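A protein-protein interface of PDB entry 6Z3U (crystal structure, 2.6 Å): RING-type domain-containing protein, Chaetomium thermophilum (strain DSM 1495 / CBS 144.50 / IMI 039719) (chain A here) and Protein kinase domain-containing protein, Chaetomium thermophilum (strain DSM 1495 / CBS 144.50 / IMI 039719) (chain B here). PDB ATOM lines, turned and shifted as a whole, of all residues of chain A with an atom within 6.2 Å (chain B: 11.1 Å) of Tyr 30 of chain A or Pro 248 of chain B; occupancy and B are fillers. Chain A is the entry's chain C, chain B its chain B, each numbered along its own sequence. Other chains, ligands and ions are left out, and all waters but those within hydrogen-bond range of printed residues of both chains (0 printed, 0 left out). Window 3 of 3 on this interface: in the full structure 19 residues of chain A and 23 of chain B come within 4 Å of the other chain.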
ATOM      1  N   SER A  26     -15.807  -0.332  15.460  1.00  0.00           N
ATOM      2  CA  SER A  26     -15.145  -1.155  14.454  1.00  0.00           C
ATOM      3  C   SER A  26     -13.886  -0.482  13.922  1.00  0.00           C
ATOM      4  O   SER A  26     -12.962  -1.167  13.468  1.00  0.00           O
ATOM      5  CB  SER A  26     -16.111  -1.459  13.307  1.00  0.00           C
ATOM      6  OG  SER A  26     -16.450  -0.282  12.595  1.00  0.00           O
ATOM      7  N   LEU A  27     -13.832   0.853  13.961  1.00  0.00           N
ATOM      8  CA  LEU A  27     -12.634   1.554  13.513  1.00  0.00           C
ATOM      9  C   LEU A  27     -11.497   1.426  14.517  1.00  0.00           C
ATOM     10  O   LEU A  27     -10.326   1.398  14.126  1.00  0.00           O
ATOM     11  CB  LEU A  27     -12.942   3.033  13.278  1.00  0.00           C
ATOM     12  CG  LEU A  27     -13.774   3.401  12.052  1.00  0.00           C
ATOM     13  CD1 LEU A  27     -14.004   4.902  12.008  1.00  0.00           C
ATOM     14  CD2 LEU A  27     -13.090   2.931  10.782  1.00  0.00           C
ATOM     15  N   ASP A  28     -11.826   1.347  15.809  1.00  0.00           N
ATOM     16  CA  ASP A  28     -10.800   1.328  16.846  1.00  0.00           C
ATOM     17  C   ASP A  28      -9.730   0.278  16.579  1.00  0.00           C
ATOM     18  O   ASP A  28      -8.554   0.498  16.891  1.00  0.00           O
ATOM     19  CB  ASP A  28     -11.451   1.086  18.211  1.00  0.00           C
ATOM     20  CG  ASP A  28     -12.474   2.153  18.566  1.00  0.00           C
ATOM     21  OD1 ASP A  28     -12.520   3.191  17.868  1.00  0.00           O
ATOM     22  OD2 ASP A  28     -13.230   1.951  19.542  1.00  0.00           O
ATOM     23  N   LYS A  29     -10.106  -0.863  15.992  1.00  0.00           N
ATOM     24  CA  LYS A  29      -9.123  -1.917  15.762  1.00  0.00           C
ATOM     25  C   LYS A  29      -8.026  -1.441  14.817  1.00  0.00           C
ATOM     26  O   LYS A  29      -6.847  -1.765  15.005  1.00  0.00           O
ATOM     27  CB  LYS A  29      -9.784  -3.174  15.186  1.00  0.00           C
ATOM     28  CG  LYS A  29     -11.286  -3.312  15.406  1.00  0.00           C
ATOM     29  CD  LYS A  29     -11.783  -4.698  15.003  1.00  0.00           C
ATOM     30  CE  LYS A  29     -11.652  -4.949  13.505  1.00  0.00           C
ATOM     31  NZ  LYS A  29     -12.690  -4.241  12.711  1.00  0.00           N
ATOM     32  N   TYR A  30      -8.398  -0.666  13.799  1.00  0.00           N
ATOM     33  CA  TYR A  30      -7.461  -0.245  12.765  1.00  0.00           C
ATOM     34  C   TYR A  30      -6.689   1.012  13.142  1.00  0.00           C
ATOM     35  O   TYR A  30      -5.518   1.142  12.765  1.00  0.00           O
ATOM     36  CB  TYR A  30      -8.212  -0.015  11.451  1.00  0.00           C
ATOM     37  CG  TYR A  30      -8.962  -1.235  10.964  1.00  0.00           C
ATOM     38  CD1 TYR A  30      -8.302  -2.254  10.292  1.00  0.00           C
ATOM     39  CD2 TYR A  30     -10.326  -1.368  11.178  1.00  0.00           C
ATOM     40  CE1 TYR A  30      -8.980  -3.372   9.844  1.00  0.00           C
ATOM     41  CE2 TYR A  30     -11.015  -2.482  10.734  1.00  0.00           C
ATOM     42  CZ  TYR A  30     -10.336  -3.484  10.067  1.00  0.00           C
ATOM     43  OH  TYR A  30     -11.011  -4.599   9.620  1.00  0.00           O
ATOM     44  N   ARG A  31      -7.308   1.935  13.885  1.00  0.00           N
ATOM     45  CA  ARG A  31      -6.611   3.158  14.269  1.00  0.00           C
ATOM     46  C   ARG A  31      -5.302   2.854  14.984  1.00  0.00           C
ATOM     47  O   ARG A  31      -4.353   3.642  14.904  1.00  0.00           O
ATOM     48  CB  ARG A  31      -7.509   4.021  15.158  1.00  0.00           C
ATOM     49  CG  ARG A  31      -8.870   4.335  14.558  1.00  0.00           C
ATOM     50  CD  ARG A  31      -9.610   5.389  15.371  1.00  0.00           C
ATOM     51  NE  ARG A  31      -9.560   6.702  14.730  1.00  0.00           N
ATOM     52  CZ  ARG A  31     -10.576   7.278  14.085  1.00  0.00           C
ATOM     53  NH1 ARG A  31     -11.754   6.672  13.988  1.00  0.00           N
ATOM     54  NH2 ARG A  31     -10.411   8.474  13.538  1.00  0.00           N
ATOM     55  N   ILE A  32      -5.227   1.718  15.681  1.00  0.00           N
ATOM     56  CA  ILE A  32      -4.016   1.308  16.381  1.00  0.00           C
ATOM     57  C   ILE A  32      -3.234   0.258  15.598  1.00  0.00           C
ATOM     58  O   ILE A  32      -2.256  -0.292  16.112  1.00  0.00           O
ATOM     59  CB  ILE A  32      -4.332   0.799  17.800  1.00  0.00           C
ATOM     60  CG1 ILE A  32      -5.385  -0.311  17.759  1.00  0.00           C
ATOM     61  CG2 ILE A  32      -4.787   1.951  18.686  1.00  0.00           C
ATOM     62  CD1 ILE A  32      -5.783  -0.823  19.130  1.00  0.00           C
ATOM     63  N   ASP A  33      -3.647  -0.038  14.369  1.00  0.00           N
ATOM     64  CA  ASP A  33      -2.859  -0.916  13.514  1.00  0.00           C
ATOM     65  C   ASP A  33      -1.644  -0.155  12.997  1.00  0.00           C
ATOM     66  O   ASP A  33      -1.778   0.924  12.412  1.00  0.00           O
ATOM     67  CB  ASP A  33      -3.703  -1.427  12.351  1.00  0.00           C
ATOM     68  CG  ASP A  33      -2.931  -2.364  11.444  1.00  0.00           C
ATOM     69  OD1 ASP A  33      -1.818  -2.779  11.827  1.00  0.00           O
ATOM     70  OD2 ASP A  33      -3.435  -2.684  10.347  1.00  0.00           O
ATOM     71  N   GLN A  34      -0.455  -0.716  13.226  1.00  0.00           N
ATOM     72  CA  GLN A  34       0.770  -0.032  12.824  1.00  0.00           C
ATOM     73  C   GLN A  34       0.755   0.305  11.337  1.00  0.00           C
ATOM     74  O   GLN A  34       1.157   1.404  10.937  1.00  0.00           O
ATOM     75  CB  GLN A  34       1.986  -0.894  13.165  1.00  0.00           C
ATOM     76  CG  GLN A  34       3.308  -0.152  13.087  1.00  0.00           C
ATOM     77  CD  GLN A  34       3.428   0.934  14.142  1.00  0.00           C
ATOM     78  OE1 GLN A  34       3.605   2.108  13.821  1.00  0.00           O
ATOM     79  NE2 GLN A  34       3.333   0.544  15.410  1.00  0.00           N
ATOM     80  N   HIS A  36      -1.735   0.885   9.309  1.00  0.00           N
ATOM     81  CA  HIS A  36      -2.682   1.920   8.907  1.00  0.00           C
ATOM     82  C   HIS A  36      -2.176   3.308   9.274  1.00  0.00           C
ATOM     83  O   HIS A  36      -2.301   4.250   8.485  1.00  0.00           O
ATOM     84  CB  HIS A  36      -4.041   1.674   9.556  1.00  0.00           C
ATOM     85  CG  HIS A  36      -4.840   0.600   8.891  1.00  0.00           C
ATOM     86  ND1 HIS A  36      -4.477  -0.729   8.930  1.00  0.00           N
ATOM     87  CD2 HIS A  36      -5.986   0.657   8.173  1.00  0.00           C
ATOM     88  CE1 HIS A  36      -5.365  -1.444   8.265  1.00  0.00           C
ATOM     89  NE2 HIS A  36      -6.289  -0.627   7.794  1.00  0.00           N
ATOM     90  N   ILE A  37      -1.604   3.456  10.467  1.00  0.00           N
ATOM     91  CA  ILE A  37      -1.123   4.764  10.896  1.00  0.00           C
ATOM     92  C   ILE A  37       0.174   5.118  10.182  1.00  0.00           C
ATOM     93  O   ILE A  37       0.276   6.166   9.532  1.00  0.00           O
ATOM     94  CB  ILE A  37      -0.964   4.801  12.431  1.00  0.00           C
ATOM     95  CG1 ILE A  37       0.001   3.713  12.916  1.00  0.00           C
ATOM     96  CG2 ILE A  37      -2.326   4.654  13.097  1.00  0.00           C
ATOM     97  CD1 ILE A  37      -0.139   3.370  14.388  1.00  0.00           C
ATOM     98  N   TYR A  41      -3.162   5.922   6.270  1.00  0.00           N
ATOM     99  CA  TYR A  41      -4.581   5.734   6.004  1.00  0.00           C
ATOM    100  C   TYR A  41      -5.385   6.796   6.742  1.00  0.00           C
ATOM    101  O   TYR A  41      -5.181   7.024   7.939  1.00  0.00           O
ATOM    102  CB  TYR A  41      -5.043   4.342   6.430  1.00  0.00           C
ATOM    103  CG  TYR A  41      -6.489   4.078   6.068  1.00  0.00           C
ATOM    104  CD1 TYR A  41      -7.521   4.489   6.904  1.00  0.00           C
ATOM    105  CD2 TYR A  41      -6.824   3.438   4.884  1.00  0.00           C
ATOM    106  CE1 TYR A  41      -8.843   4.262   6.574  1.00  0.00           C
ATOM    107  CE2 TYR A  41      -8.144   3.206   4.545  1.00  0.00           C
ATOM    108  CZ  TYR A  41      -9.149   3.622   5.394  1.00  0.00           C
ATOM    109  OH  TYR A  41     -10.466   3.396   5.068  1.00  0.00           O
ATOM    110  N   PHE A  43      -8.655   7.929   8.357  1.00  0.00           N
ATOM    111  CA  PHE A  43      -9.958   7.550   8.886  1.00  0.00           C
ATOM    112  C   PHE A  43     -10.961   8.687   8.759  1.00  0.00           C
ATOM    113  O   PHE A  43     -12.167   8.438   8.663  1.00  0.00           O
ATOM    114  CB  PHE A  43      -9.828   7.115  10.345  1.00  0.00           C
ATOM    115  CG  PHE A  43      -8.991   5.884  10.530  1.00  0.00           C
ATOM    116  CD1 PHE A  43      -9.577   4.631  10.550  1.00  0.00           C
ATOM    117  CD2 PHE A  43      -7.618   5.977  10.676  1.00  0.00           C
ATOM    118  CE1 PHE A  43      -8.811   3.496  10.718  1.00  0.00           C
ATOM    119  CE2 PHE A  43      -6.847   4.845  10.842  1.00  0.00           C
ATOM    120  CZ  PHE A  43      -7.444   3.603  10.863  1.00  0.00           C
ATOM    121  N   TYR A  46     -12.795   8.244   5.541  1.00  0.00           N
ATOM    122  CA  TYR A  46     -13.805   7.189   5.600  1.00  0.00           C
ATOM    123  C   TYR A  46     -15.079   7.689   6.271  1.00  0.00           C
ATOM    124  O   TYR A  46     -16.187   7.470   5.768  1.00  0.00           O
ATOM    125  CB  TYR A  46     -13.250   5.968   6.337  1.00  0.00           C
ATOM    126  CG  TYR A  46     -14.279   4.887   6.599  1.00  0.00           C
ATOM    127  CD1 TYR A  46     -14.590   3.951   5.621  1.00  0.00           C
ATOM    128  CD2 TYR A  46     -14.931   4.796   7.822  1.00  0.00           C
ATOM    129  CE1 TYR A  46     -15.524   2.959   5.850  1.00  0.00           C
ATOM    130  CE2 TYR A  46     -15.868   3.805   8.060  1.00  0.00           C
ATOM    131  CZ  TYR A  46     -16.160   2.888   7.070  1.00  0.00           C
ATOM    132  OH  TYR A  46     -17.089   1.895   7.296  1.00  0.00           O
ATOM    133  N   ARG B 243      -8.401   4.262  -8.358  1.00  0.00           N
ATOM    134  CA  ARG B 243      -9.154   3.380  -7.480  1.00  0.00           C
ATOM    135  C   ARG B 243      -9.901   4.215  -6.452  1.00  0.00           C
ATOM    136  O   ARG B 243      -9.421   5.266  -6.019  1.00  0.00           O
ATOM    137  CB  ARG B 243      -8.225   2.384  -6.772  1.00  0.00           C
ATOM    138  CG  ARG B 243      -8.935   1.224  -6.093  1.00  0.00           C
ATOM    139  CD  ARG B 243      -8.294   0.884  -4.757  1.00  0.00           C
ATOM    140  NE  ARG B 243      -8.707  -0.428  -4.268  1.00  0.00           N
ATOM    141  CZ  ARG B 243      -9.867  -0.676  -3.664  1.00  0.00           C
ATOM    142  NH1 ARG B 243     -10.747   0.300  -3.475  1.00  0.00           N
ATOM    143  NH2 ARG B 243     -10.151  -1.906  -3.253  1.00  0.00           N
ATOM    144  N   SER B 244     -11.079   3.732  -6.067  1.00  0.00           N
ATOM    145  CA  SER B 244     -11.859   4.390  -5.030  1.00  0.00           C
ATOM    146  C   SER B 244     -11.184   4.215  -3.675  1.00  0.00           C
ATOM    147  O   SER B 244     -10.467   3.239  -3.435  1.00  0.00           O
ATOM    148  CB  SER B 244     -13.276   3.818  -4.977  1.00  0.00           C
ATOM    149  OG  SER B 244     -13.996   4.118  -6.162  1.00  0.00           O
ATOM    150  N   PHE B 245     -11.437   5.161  -2.777  1.00  0.00           N
ATOM    151  CA  PHE B 245     -10.894   5.080  -1.429  1.00  0.00           C
ATOM    152  C   PHE B 245     -11.255   3.748  -0.786  1.00  0.00           C
ATOM    153  O   PHE B 245     -12.435   3.417  -0.636  1.00  0.00           O
ATOM    154  CB  PHE B 245     -11.417   6.236  -0.574  1.00  0.00           C
ATOM    155  CG  PHE B 245     -10.820   7.572  -0.915  1.00  0.00           C
ATOM    156  CD1 PHE B 245     -10.037   7.742  -2.044  1.00  0.00           C
ATOM    157  CD2 PHE B 245     -11.035   8.659  -0.087  1.00  0.00           C
ATOM    158  CE1 PHE B 245      -9.491   8.974  -2.345  1.00  0.00           C
ATOM    159  CE2 PHE B 245     -10.488   9.892  -0.380  1.00  0.00           C
ATOM    160  CZ  PHE B 245      -9.716  10.050  -1.511  1.00  0.00           C
ATOM    161  N   ALA B 246     -10.235   2.988  -0.400  1.00  0.00           N
ATOM    162  CA  ALA B 246     -10.460   1.698   0.233  1.00  0.00           C
ATOM    163  C   ALA B 246     -10.944   1.877   1.667  1.00  0.00           C
ATOM    164  O   ALA B 246     -10.645   2.872   2.329  1.00  0.00           O
ATOM    165  CB  ALA B 246      -9.179   0.867   0.219  1.00  0.00           C
ATOM    166  N   ASP B 247     -11.700   0.897   2.143  1.00  0.00           N
ATOM    167  CA  ASP B 247     -12.148   0.907   3.524  1.00  0.00           C
ATOM    168  C   ASP B 247     -11.013   0.487   4.450  1.00  0.00           C
ATOM    169  O   ASP B 247      -9.994  -0.044   4.002  1.00  0.00           O
ATOM    170  CB  ASP B 247     -13.337  -0.028   3.700  1.00  0.00           C
ATOM    171  CG  ASP B 247     -14.623   0.553   3.149  1.00  0.00           C
ATOM    172  OD1 ASP B 247     -14.602   1.717   2.699  1.00  0.00           O
ATOM    173  OD2 ASP B 247     -15.658  -0.146   3.183  1.00  0.00           O
ATOM    174  N   PRO B 248     -11.154   0.735   5.751  1.00  0.00           N
ATOM    175  CA  PRO B 248     -10.116   0.300   6.694  1.00  0.00           C
ATOM    176  C   PRO B 248      -9.977  -1.215   6.691  1.00  0.00           C
ATOM    177  O   PRO B 248     -10.964  -1.948   6.781  1.00  0.00           O
ATOM    178  CB  PRO B 248     -10.615   0.826   8.045  1.00  0.00           C
ATOM    179  CG  PRO B 248     -11.558   1.928   7.701  1.00  0.00           C
ATOM    180  CD  PRO B 248     -12.210   1.514   6.418  1.00  0.00           C
ATOM    181  N   GLY B 249      -8.734  -1.679   6.590  1.00  0.00           N
ATOM    182  CA  GLY B 249      -8.437  -3.088   6.503  1.00  0.00           C
ATOM    183  C   GLY B 249      -8.411  -3.639   5.095  1.00  0.00           C
ATOM    184  O   GLY B 249      -7.991  -4.788   4.903  1.00  0.00           O
ATOM    185  N   ARG B 250      -8.830  -2.852   4.107  1.00  0.00           N
ATOM    186  CA  ARG B 250      -8.846  -3.276   2.711  1.00  0.00           C
ATOM    187  C   ARG B 250      -7.483  -2.954   2.112  1.00  0.00           C
ATOM    188  O   ARG B 250      -7.115  -1.781   1.983  1.00  0.00           O
ATOM    189  CB  ARG B 250      -9.970  -2.574   1.955  1.00  0.00           C
ATOM    190  CG  ARG B 250     -10.103  -2.973   0.488  1.00  0.00           C
ATOM    191  CD  ARG B 250     -10.239  -4.479   0.328  1.00  0.00           C
ATOM    192  NE  ARG B 250     -11.225  -5.034   1.253  1.00  0.00           N
ATOM    193  CZ  ARG B 250     -12.495  -5.287   0.946  1.00  0.00           C
ATOM    194  NH1 ARG B 250     -12.962  -5.045  -0.274  1.00  0.00           N
ATOM    195  NH2 ARG B 250     -13.303  -5.788   1.870  1.00  0.00           N
ATOM    196  N   ARG B 251      -6.735  -3.992   1.746  1.00  0.00           N
ATOM    197  CA  ARG B 251      -5.367  -3.811   1.284  1.00  0.00           C
ATOM    198  C   ARG B 251      -5.365  -3.264  -0.137  1.00  0.00           C
ATOM    199  O   ARG B 251      -6.223  -3.613  -0.954  1.00  0.00           O
ATOM    200  CB  ARG B 251      -4.602  -5.134   1.344  1.00  0.00           C
ATOM    201  CG  ARG B 251      -4.687  -5.813   2.703  1.00  0.00           C
ATOM    202  CD  ARG B 251      -3.886  -7.102   2.776  1.00  0.00           C
ATOM    203  NE  ARG B 251      -2.468  -6.823   2.992  1.00  0.00           N
ATOM    204  CZ  ARG B 251      -1.914  -6.679   4.197  1.00  0.00           C
ATOM    205  NH1 ARG B 251      -2.655  -6.791   5.293  1.00  0.00           N
ATOM    206  NH2 ARG B 251      -0.618  -6.418   4.312  1.00  0.00           N
ATOM    207  N   MET B 252      -4.400  -2.396  -0.424  1.00  0.00           N
ATOM    208  CA  MET B 252      -4.212  -1.832  -1.752  1.00  0.00           C
ATOM    209  C   MET B 252      -2.845  -2.235  -2.286  1.00  0.00           C
ATOM    210  O   MET B 252      -1.977  -2.711  -1.550  1.00  0.00           O
ATOM    211  CB  MET B 252      -4.330  -0.304  -1.732  1.00  0.00           C
ATOM    212  CG  MET B 252      -5.745   0.219  -1.596  1.00  0.00           C
ATOM    213  SD  MET B 252      -5.747   1.959  -1.123  1.00  0.00           S
ATOM    214  CE  MET B 252      -7.184   2.555  -2.005  1.00  0.00           C
ATOM    215  N   ARG B 271       0.297  -0.856   2.194  1.00  0.00           N
ATOM    216  CA  ARG B 271      -0.950  -1.418   1.701  1.00  0.00           C
ATOM    217  C   ARG B 271      -2.184  -0.666   2.177  1.00  0.00           C
ATOM    218  O   ARG B 271      -3.282  -0.944   1.683  1.00  0.00           O
ATOM    219  CB  ARG B 271      -1.076  -2.888   2.134  1.00  0.00           C
ATOM    220  CG  ARG B 271       0.194  -3.707   1.962  1.00  0.00           C
ATOM    221  CD  ARG B 271       0.473  -4.011   0.500  1.00  0.00           C
ATOM    222  NE  ARG B 271      -0.510  -4.933  -0.061  1.00  0.00           N
ATOM    223  CZ  ARG B 271      -0.482  -5.389  -1.309  1.00  0.00           C
ATOM    224  NH1 ARG B 271      -1.420  -6.226  -1.728  1.00  0.00           N
ATOM    225  NH2 ARG B 271       0.482  -5.009  -2.139  1.00  0.00           N
ATOM    226  N   HIS B 272      -2.040   0.263   3.126  1.00  0.00           N
ATOM    227  CA  HIS B 272      -3.162   1.033   3.675  1.00  0.00           C
ATOM    228  C   HIS B 272      -2.769   2.507   3.651  1.00  0.00           C
ATOM    229  O   HIS B 272      -2.315   3.057   4.657  1.00  0.00           O
ATOM    230  CB  HIS B 272      -3.510   0.552   5.083  1.00  0.00           C
ATOM    231  CG  HIS B 272      -3.936  -0.882   5.142  1.00  0.00           C
ATOM    232  ND1 HIS B 272      -3.336  -1.802   5.976  1.00  0.00           N
ATOM    233  CD2 HIS B 272      -4.905  -1.554   4.478  1.00  0.00           C
ATOM    234  CE1 HIS B 272      -3.911  -2.980   5.815  1.00  0.00           C
ATOM    235  NE2 HIS B 272      -4.869  -2.856   4.915  1.00  0.00           N
ATOM    236  N   TYR B 273      -2.954   3.143   2.501  1.00  0.00           N
ATOM    237  CA  TYR B 273      -2.587   4.536   2.290  1.00  0.00           C
ATOM    238  C   TYR B 273      -3.820   5.351   1.907  1.00  0.00           C
ATOM    239  O   TYR B 273      -4.939   4.838   1.844  1.00  0.00           O
ATOM    240  CB  TYR B 273      -1.503   4.648   1.214  1.00  0.00           C
ATOM    241  CG  TYR B 273      -1.828   3.934  -0.082  1.00  0.00           C
ATOM    242  CD1 TYR B 273      -2.578   4.556  -1.071  1.00  0.00           C
ATOM    243  CD2 TYR B 273      -1.376   2.643  -0.322  1.00  0.00           C
ATOM    244  CE1 TYR B 273      -2.872   3.911  -2.261  1.00  0.00           C
ATOM    245  CE2 TYR B 273      -1.665   1.989  -1.508  1.00  0.00           C
ATOM    246  CZ  TYR B 273      -2.413   2.628  -2.472  1.00  0.00           C
ATOM    247  OH  TYR B 273      -2.698   1.978  -3.651  1.00  0.00           O
ATOM    248  N   GLY B 274      -3.603   6.640   1.652  1.00  0.00           N
ATOM    249  CA  GLY B 274      -4.687   7.546   1.332  1.00  0.00           C
ATOM    250  C   GLY B 274      -4.320   8.583   0.291  1.00  0.00           C
ATOM    251  O   GLY B 274      -3.422   8.363  -0.526  1.00  0.00           O
ATOM    252  N   LYS B 369       1.153  11.325   6.908  1.00  0.00           N
ATOM    253  CA  LYS B 369       0.209  11.911   7.851  1.00  0.00           C
ATOM    254  C   LYS B 369       0.411  13.415   7.993  1.00  0.00           C
ATOM    255  O   LYS B 369      -0.565  14.155   8.160  1.00  0.00           O
ATOM    256  CB  LYS B 369       0.342  11.218   9.207  1.00  0.00           C
ATOM    257  CG  LYS B 369      -0.018   9.739   9.175  1.00  0.00           C
ATOM    258  CD  LYS B 369       0.243   9.062  10.510  1.00  0.00           C
ATOM    259  CE  LYS B 369       1.728   8.801  10.731  1.00  0.00           C
ATOM    260  NZ  LYS B 369       2.028   8.300  12.111  1.00  0.00           N
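O of Ala 246 of chain B sits at hydrogen-bond distance from OH of Tyr 41 of chain A, at 2.8 Å.
The backbone carbonyl oxygen (O) of His 272 of chain B sits at hydrogen-bond distance from the backbone NH (N) of Tyr 41 of chain A, 3.4 Å away.
The backbone nitrogen of Pro 248 of chain B lies close to the side-chain hydroxyl of Tyr 41 of chain A, 2.8 Å away.
The backbone NH of Gly 249 of chain B lies within hydrogen-bond range of a ring nitrogen (NE2) of His 36 of chain A.
ND1 of His 272 of chain B lies close to ND1 of His 36 of chain A (3.3 Å).
A ring nitrogen (ND1) of His 36 of chain A lies within hydrogen-bond range of the side-chain carboxylate (OD2) of Asp 33 of chain A.
O of His 36 of chain A sits at hydrogen-bond distance from N of Tyr 41 of chain A (2.9 Å).
Tyr 30 of chain A touches two residues of chain B.
Of chain A, only Leu 27, Tyr 30, His 36, Tyr 41 and Tyr 46 come within 4 Å of Pro 248 of chain B.
No residue of chain B comes within 4 Å of Ser 26 of chain A.
Leu 27 of chain A touches one residue of chain B.
Lys 29 of chain A touches none of the printed residues of chain B.
No residue of chain B comes within 4 Å of Asp 33 of chain A.
His 36 of chain A touches just these residues of chain B: Pro 248, Gly 249 and His 272.
No residue of chain B comes within 4 Å of Phe 43 of chain A.
Of the printed residues of chain A, Gly 249 of chain B touches Tyr 30 and His 36.
Printed residues of chain A within 4 Å of Lys 369 of chain B: Ile 37 (3.1 Å).
Of the printed residues of chain A, Tyr 273 of chain B touches Tyr 41.
Among the printed residues, merely in contact across the chains: Leu 27 of chain A with Pro 248 of chain B (3.6 Å), Tyr 30 of chain A with Pro 248 of chain B (3.7 Å), Tyr 30 of chain A with Gly 249 of chain B (3.4 Å), His 36 of chain A with Pro 248 of chain B (3.9 Å), Ile 37 of chain A with Lys 369 of chain B (3.1 Å), Tyr 41 of chain A with Asp 247 of chain B (3.0 Å), Tyr 41 of chain A with Tyr 273 of chain B (3.8 Å), Tyr 46 of chain A with Asp 247 of chain B (3.5 Å) and Tyr 46 of chain A with Pro 248 of chain B (3.5 Å).
Hydrophobic or aromatic side chains of chain B that line the printed part of chain A: Pro 248 and His 272.
Among the printed residues, 14 pairs touch across the chains.
Among the printed residues, no Asp or Glu carboxylate lies within 4 Å of a Lys or Arg side-chain nitrogen of the other chain.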
